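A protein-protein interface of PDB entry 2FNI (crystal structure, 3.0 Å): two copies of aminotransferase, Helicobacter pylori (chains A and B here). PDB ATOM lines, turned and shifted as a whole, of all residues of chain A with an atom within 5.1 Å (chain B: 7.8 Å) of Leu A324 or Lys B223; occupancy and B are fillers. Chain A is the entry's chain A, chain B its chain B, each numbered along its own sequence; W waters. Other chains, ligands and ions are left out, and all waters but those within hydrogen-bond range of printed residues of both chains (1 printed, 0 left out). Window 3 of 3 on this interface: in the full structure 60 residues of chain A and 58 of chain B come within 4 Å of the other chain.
Printed residues of chain B within 4 Å of Leu A92: Ile B225 (3.96 Å). Of chain B, only Val B222, Lys B223, Ser B224 and Ile B225 come within 4 Å of Leu A324. Tyr A325 touches none of the printed residues of chain B. Of the printed residues of chain A, His B210 touches Asn A89. Gly B211 touches none of the printed residues of chain A. Printed residues of chain A within 4 Å of Met B212: Tyr A322 (3.7 Å). Printed residues of chain A within 4 Å of Glu B221: Tyr A322 and Gln A323. The nearest printed residue of chain B that does not touch Tyr A322 is Lys B223 (6.0 Å).
OH of Tyr A325 lies within hydrogen-bond range of ND2 of Asn A89. O of Leu B213 lies within hydrogen-bond range of N of Glu B221, 2.8 Å away.
O of His B210 sits close to OD1 of Asn A89 (3.3 Å). The backbone NH (N) of Gln A323 lies within hydrogen-bond range of the side-chain carboxylate (OE2) of Glu B221, 2.7 Å away. The backbone NH (N) of Leu A324 is in hydrogen-bond range of the backbone carbonyl oxygen (O) of Val B222 (2.8 Å).
Water W1 lies within hydrogen-bond range of O of Gly B226, ND1 of His B210 and OD1 of Asn A89.
No position is printed for both chains.
Asn A89 touches Ile B225 (ND2 to CG2, 3.7 Å). Gly B226 touches Asn A89. CD1 of Leu A92 touches CG2 of Ile B225, 3.96 Å away. Tyr A322 touches Met B212. Gly B220 touches Tyr A322. OE2 of Glu B221 touches C of Tyr A322 (3.6 Å). Gln A323 touches Val B222 (N to O, 3.7 Å). Gln A323 touches Lys B223. O of Lys B223 touches CD1 of Leu A324, at 3.6 Å. Leu A324 touches Ile B225 (CD2 to N, 3.8 Å).
Hydrophobic or aromatic side chains of chain A that line the printed part of chain B: Leu A92, Tyr A322 and Leu A324. Of the 12 printed residues of chain B, 9 touch a printed residue of chain A. Printed residues of chain B that touch a printed residue of chain A: His B210, Met B212, Gly B220, Glu B221, Val B222, Lys B223, Ser B224, Ile B225 and Gly B226. Among the printed residues, 15 pairs touch across the chains. Among the printed residues, no Asp or Glu carboxylate lies within 4 Å of a Lys or Arg side-chain nitrogen of the other chain.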
ATOM      1  N   ASN A  89      28.753  13.778   0.780  1.00  0.00           N
ATOM      2  CA  ASN A  89      28.592  13.066   2.048  1.00  0.00           C
ATOM      3  C   ASN A  89      29.810  13.196   2.952  1.00  0.00           C
ATOM      4  O   ASN A  89      29.679  13.336   4.166  1.00  0.00           O
ATOM      5  CB  ASN A  89      28.282  11.596   1.824  1.00  0.00           C
ATOM      6  CG  ASN A  89      26.841  11.362   1.475  1.00  0.00           C
ATOM      7  OD1 ASN A  89      26.439  10.232   1.205  1.00  0.00           O
ATOM      8  ND2 ASN A  89      26.049  12.428   1.475  1.00  0.00           N
ATOM      9  N   LEU A  92      29.904  16.581   4.637  1.00  0.00           N
ATOM     10  CA  LEU A  92      29.059  16.542   5.832  1.00  0.00           C
ATOM     11  C   LEU A  92      29.782  15.862   6.992  1.00  0.00           C
ATOM     12  O   LEU A  92      29.881  16.416   8.084  1.00  0.00           O
ATOM     13  CB  LEU A  92      27.721  15.858   5.549  1.00  0.00           C
ATOM     14  CG  LEU A  92      26.734  16.725   4.768  1.00  0.00           C
ATOM     15  CD1 LEU A  92      25.571  15.888   4.264  1.00  0.00           C
ATOM     16  CD2 LEU A  92      26.253  17.881   5.624  1.00  0.00           C
ATOM     17  N   TYR A 322      18.586  14.874  -3.029  1.00  0.00           N
ATOM     18  CA  TYR A 322      18.451  13.771  -2.093  1.00  0.00           C
ATOM     19  C   TYR A 322      17.748  14.215  -0.819  1.00  0.00           C
ATOM     20  O   TYR A 322      18.079  15.261  -0.240  1.00  0.00           O
ATOM     21  CB  TYR A 322      19.807  13.173  -1.749  1.00  0.00           C
ATOM     22  CG  TYR A 322      20.351  12.304  -2.838  1.00  0.00           C
ATOM     23  CD1 TYR A 322      19.659  11.175  -3.262  1.00  0.00           C
ATOM     24  CD2 TYR A 322      21.564  12.604  -3.444  1.00  0.00           C
ATOM     25  CE1 TYR A 322      20.161  10.373  -4.261  1.00  0.00           C
ATOM     26  CE2 TYR A 322      22.074  11.807  -4.442  1.00  0.00           C
ATOM     27  CZ  TYR A 322      21.369  10.701  -4.849  1.00  0.00           C
ATOM     28  OH  TYR A 322      21.885   9.928  -5.855  1.00  0.00           O
ATOM     29  N   GLN A 323      16.792  13.405  -0.379  1.00  0.00           N
ATOM     30  CA  GLN A 323      16.007  13.720   0.803  1.00  0.00           C
ATOM     31  C   GLN A 323      16.843  14.298   1.947  1.00  0.00           C
ATOM     32  O   GLN A 323      16.443  15.279   2.571  1.00  0.00           O
ATOM     33  CB  GLN A 323      15.237  12.491   1.277  1.00  0.00           C
ATOM     34  CG  GLN A 323      13.991  12.828   2.067  1.00  0.00           C
ATOM     35  CD  GLN A 323      13.552  11.681   2.938  1.00  0.00           C
ATOM     36  OE1 GLN A 323      13.874  11.631   4.124  1.00  0.00           O
ATOM     37  NE2 GLN A 323      12.833  10.737   2.355  1.00  0.00           N
ATOM     38  N   LEU A 324      17.996  13.701   2.221  1.00  0.00           N
ATOM     39  CA  LEU A 324      18.865  14.186   3.299  1.00  0.00           C
ATOM     40  C   LEU A 324      19.275  15.655   3.116  1.00  0.00           C
ATOM     41  O   LEU A 324      19.328  16.415   4.090  1.00  0.00           O
ATOM     42  CB  LEU A 324      20.116  13.304   3.444  1.00  0.00           C
ATOM     43  CG  LEU A 324      21.215  13.822   4.376  1.00  0.00           C
ATOM     44  CD1 LEU A 324      20.741  13.811   5.814  1.00  0.00           C
ATOM     45  CD2 LEU A 324      22.481  13.007   4.220  1.00  0.00           C
ATOM     46  N   TYR A 325      19.569  16.047   1.878  1.00  0.00           N
ATOM     47  CA  TYR A 325      20.044  17.401   1.621  1.00  0.00           C
ATOM     48  C   TYR A 325      18.912  18.413   1.677  1.00  0.00           C
ATOM     49  O   TYR A 325      19.081  19.513   2.199  1.00  0.00           O
ATOM     50  CB  TYR A 325      20.821  17.463   0.308  1.00  0.00           C
ATOM     51  CG  TYR A 325      22.175  16.815   0.450  1.00  0.00           C
ATOM     52  CD1 TYR A 325      22.318  15.432   0.343  1.00  0.00           C
ATOM     53  CD2 TYR A 325      23.311  17.573   0.723  1.00  0.00           C
ATOM     54  CE1 TYR A 325      23.555  14.826   0.479  1.00  0.00           C
ATOM     55  CE2 TYR A 325      24.550  16.968   0.867  1.00  0.00           C
ATOM     56  CZ  TYR A 325      24.655  15.596   0.742  1.00  0.00           C
ATOM     57  OH  TYR A 325      25.872  14.991   0.894  1.00  0.00           O
ATOM     58  N   GLN A 326      17.755  18.025   1.153  1.00  0.00           N
ATOM     59  CA  GLN A 326      16.534  18.804   1.311  1.00  0.00           C
ATOM     60  C   GLN A 326      16.282  19.058   2.789  1.00  0.00           C
ATOM     61  O   GLN A 326      16.150  20.202   3.221  1.00  0.00           O
ATOM     62  CB  GLN A 326      15.340  18.061   0.706  1.00  0.00           C
ATOM     63  CG  GLN A 326      15.186  18.289  -0.781  1.00  0.00           C
ATOM     64  CD  GLN A 326      15.094  19.770  -1.129  1.00  0.00           C
ATOM     65  OE1 GLN A 326      15.989  20.334  -1.766  1.00  0.00           O
ATOM     66  NE2 GLN A 326      14.017  20.412  -0.690  1.00  0.00           N
ATOM     67  N   GLN A 327      16.224  17.968   3.545  1.00  0.00           N
ATOM     68  CA  GLN A 327      16.063  17.987   4.983  1.00  0.00           C
ATOM     69  C   GLN A 327      16.972  19.005   5.650  1.00  0.00           C
ATOM     70  O   GLN A 327      16.559  19.701   6.562  1.00  0.00           O
ATOM     71  CB  GLN A 327      16.396  16.599   5.530  1.00  0.00           C
ATOM     72  CG  GLN A 327      15.846  16.284   6.909  1.00  0.00           C
ATOM     73  CD  GLN A 327      14.353  16.022   6.874  1.00  0.00           C
ATOM     74  OE1 GLN A 327      13.802  15.632   5.837  1.00  0.00           O
ATOM     75  NE2 GLN A 327      13.682  16.244   8.009  1.00  0.00           N
ATOM     76  N   LEU A 328      18.215  19.089   5.205  1.00  0.00           N
ATOM     77  CA  LEU A 328      19.206  19.867   5.941  1.00  0.00           C
ATOM     78  C   LEU A 328      19.260  21.331   5.531  1.00  0.00           C
ATOM     79  O   LEU A 328      19.440  22.209   6.378  1.00  0.00           O
ATOM     80  CB  LEU A 328      20.599  19.233   5.840  1.00  0.00           C
ATOM     81  CG  LEU A 328      20.816  17.971   6.675  1.00  0.00           C
ATOM     82  CD1 LEU A 328      22.200  17.419   6.428  1.00  0.00           C
ATOM     83  CD2 LEU A 328      20.595  18.252   8.153  1.00  0.00           C
ATOM     84  N   LEU B 206      23.530   0.325   5.235  1.00  0.00           N
ATOM     85  CA  LEU B 206      23.491   1.588   4.512  1.00  0.00           C
ATOM     86  C   LEU B 206      24.714   2.442   4.792  1.00  0.00           C
ATOM     87  O   LEU B 206      25.345   2.928   3.871  1.00  0.00           O
ATOM     88  CB  LEU B 206      22.206   2.360   4.839  1.00  0.00           C
ATOM     89  CG  LEU B 206      20.887   1.752   4.321  1.00  0.00           C
ATOM     90  CD1 LEU B 206      19.675   2.254   5.095  1.00  0.00           C
ATOM     91  CD2 LEU B 206      20.720   2.004   2.814  1.00  0.00           C
ATOM     92  N   HIS B 210      27.306   4.545   1.379  1.00  0.00           N
ATOM     93  CA  HIS B 210      26.813   5.855   0.936  1.00  0.00           C
ATOM     94  C   HIS B 210      25.417   6.210   1.423  1.00  0.00           C
ATOM     95  O   HIS B 210      24.907   7.279   1.105  1.00  0.00           O
ATOM     96  CB  HIS B 210      26.846   5.964  -0.588  1.00  0.00           C
ATOM     97  CG  HIS B 210      28.186   5.682  -1.181  1.00  0.00           C
ATOM     98  ND1 HIS B 210      29.266   6.517  -1.003  1.00  0.00           N
ATOM     99  CD2 HIS B 210      28.625   4.657  -1.947  1.00  0.00           C
ATOM    100  CE1 HIS B 210      30.313   6.022  -1.639  1.00  0.00           C
ATOM    101  NE2 HIS B 210      29.950   4.895  -2.223  1.00  0.00           N
ATOM    102  N   GLY B 211      24.788   5.317   2.172  1.00  0.00           N
ATOM    103  CA  GLY B 211      23.410   5.532   2.569  1.00  0.00           C
ATOM    104  C   GLY B 211      22.456   5.392   1.396  1.00  0.00           C
ATOM    105  O   GLY B 211      21.288   5.783   1.491  1.00  0.00           O
ATOM    106  N   MET B 212      22.939   4.820   0.292  1.00  0.00           N
ATOM    107  CA  MET B 212      22.135   4.707  -0.929  1.00  0.00           C
ATOM    108  C   MET B 212      21.039   3.647  -0.849  1.00  0.00           C
ATOM    109  O   MET B 212      21.304   2.478  -0.571  1.00  0.00           O
ATOM    110  CB  MET B 212      23.016   4.441  -2.146  1.00  0.00           C
ATOM    111  CG  MET B 212      22.284   4.597  -3.477  1.00  0.00           C
ATOM    112  SD  MET B 212      21.846   6.313  -3.887  1.00  0.00           S
ATOM    113  CE  MET B 212      23.458   7.028  -4.184  1.00  0.00           C
ATOM    114  N   LEU B 213      19.803   4.081  -1.095  1.00  0.00           N
ATOM    115  CA  LEU B 213      18.633   3.198  -1.175  1.00  0.00           C
ATOM    116  C   LEU B 213      18.213   3.151  -2.634  1.00  0.00           C
ATOM    117  O   LEU B 213      18.256   4.181  -3.308  1.00  0.00           O
ATOM    118  CB  LEU B 213      17.494   3.777  -0.338  1.00  0.00           C
ATOM    119  CG  LEU B 213      17.685   3.798   1.178  1.00  0.00           C
ATOM    120  CD1 LEU B 213      17.265   5.137   1.791  1.00  0.00           C
ATOM    121  CD2 LEU B 213      16.930   2.613   1.804  1.00  0.00           C
ATOM    122  N   GLY B 220      18.349   6.604  -7.003  1.00  0.00           N
ATOM    123  CA  GLY B 220      18.479   6.210  -5.612  1.00  0.00           C
ATOM    124  C   GLY B 220      17.900   7.238  -4.661  1.00  0.00           C
ATOM    125  O   GLY B 220      17.367   8.261  -5.086  1.00  0.00           O
ATOM    126  N   GLU B 221      18.009   6.959  -3.366  1.00  0.00           N
ATOM    127  CA  GLU B 221      17.580   7.900  -2.341  1.00  0.00           C
ATOM    128  C   GLU B 221      18.553   7.901  -1.176  1.00  0.00           C
ATOM    129  O   GLU B 221      19.017   6.848  -0.749  1.00  0.00           O
ATOM    130  CB  GLU B 221      16.184   7.551  -1.827  1.00  0.00           C
ATOM    131  CG  GLU B 221      15.639   8.598  -0.868  1.00  0.00           C
ATOM    132  CD  GLU B 221      15.689  10.001  -1.464  1.00  0.00           C
ATOM    133  OE1 GLU B 221      14.817  10.299  -2.304  1.00  0.00           O
ATOM    134  OE2 GLU B 221      16.590  10.798  -1.105  1.00  0.00           O
ATOM    135  N   VAL B 222      18.862   9.079  -0.658  1.00  0.00           N
ATOM    136  CA  VAL B 222      19.792   9.172   0.454  1.00  0.00           C
ATOM    137  C   VAL B 222      19.181   9.938   1.629  1.00  0.00           C
ATOM    138  O   VAL B 222      19.013  11.158   1.576  1.00  0.00           O
ATOM    139  CB  VAL B 222      21.134   9.809   0.014  1.00  0.00           C
ATOM    140  CG1 VAL B 222      22.066  10.004   1.220  1.00  0.00           C
ATOM    141  CG2 VAL B 222      21.792   8.949  -1.056  1.00  0.00           C
ATOM    142  N   LYS B 223      18.848   9.209   2.689  1.00  0.00           N
ATOM    143  CA  LYS B 223      18.220   9.816   3.862  1.00  0.00           C
ATOM    144  C   LYS B 223      19.213  10.105   4.986  1.00  0.00           C
ATOM    145  O   LYS B 223      18.849  10.714   5.994  1.00  0.00           O
ATOM    146  CB  LYS B 223      17.091   8.927   4.382  1.00  0.00           C
ATOM    147  CG  LYS B 223      16.013   8.679   3.353  1.00  0.00           C
ATOM    148  CD  LYS B 223      15.005   7.646   3.822  1.00  0.00           C
ATOM    149  CE  LYS B 223      13.876   7.504   2.804  1.00  0.00           C
ATOM    150  NZ  LYS B 223      12.884   6.465   3.181  1.00  0.00           N
ATOM    151  N   SER B 224      20.462   9.678   4.800  1.00  0.00           N
ATOM    152  CA  SER B 224      21.498   9.796   5.827  1.00  0.00           C
ATOM    153  C   SER B 224      22.824   9.351   5.233  1.00  0.00           C
ATOM    154  O   SER B 224      22.846   8.520   4.306  1.00  0.00           O
ATOM    155  CB  SER B 224      21.158   8.906   7.012  1.00  0.00           C
ATOM    156  OG  SER B 224      20.690   7.665   6.529  1.00  0.00           O
ATOM    157  N   ILE B 225      23.924   9.886   5.774  1.00  0.00           N
ATOM    158  CA  ILE B 225      25.240   9.676   5.165  1.00  0.00           C
ATOM    159  C   ILE B 225      25.754   8.241   5.271  1.00  0.00           C
ATOM    160  O   ILE B 225      25.297   7.449   6.093  1.00  0.00           O
ATOM    161  CB  ILE B 225      26.321  10.661   5.675  1.00  0.00           C
ATOM    162  CG1 ILE B 225      26.439  10.588   7.191  1.00  0.00           C
ATOM    163  CG2 ILE B 225      26.034  12.067   5.203  1.00  0.00           C
ATOM    164  CD1 ILE B 225      27.259   9.410   7.662  1.00  0.00           C
ATOM    165  N   GLY B 226      26.715   7.929   4.414  1.00  0.00           N
ATOM    166  CA  GLY B 226      27.354   6.631   4.397  1.00  0.00           C
ATOM    167  C   GLY B 226      28.703   6.765   3.723  1.00  0.00           C
ATOM    168  O   GLY B 226      28.998   7.784   3.089  1.00  0.00           O
HETATM  169  O   HOH W   1      29.084   8.317   0.679  1.00  0.00           O
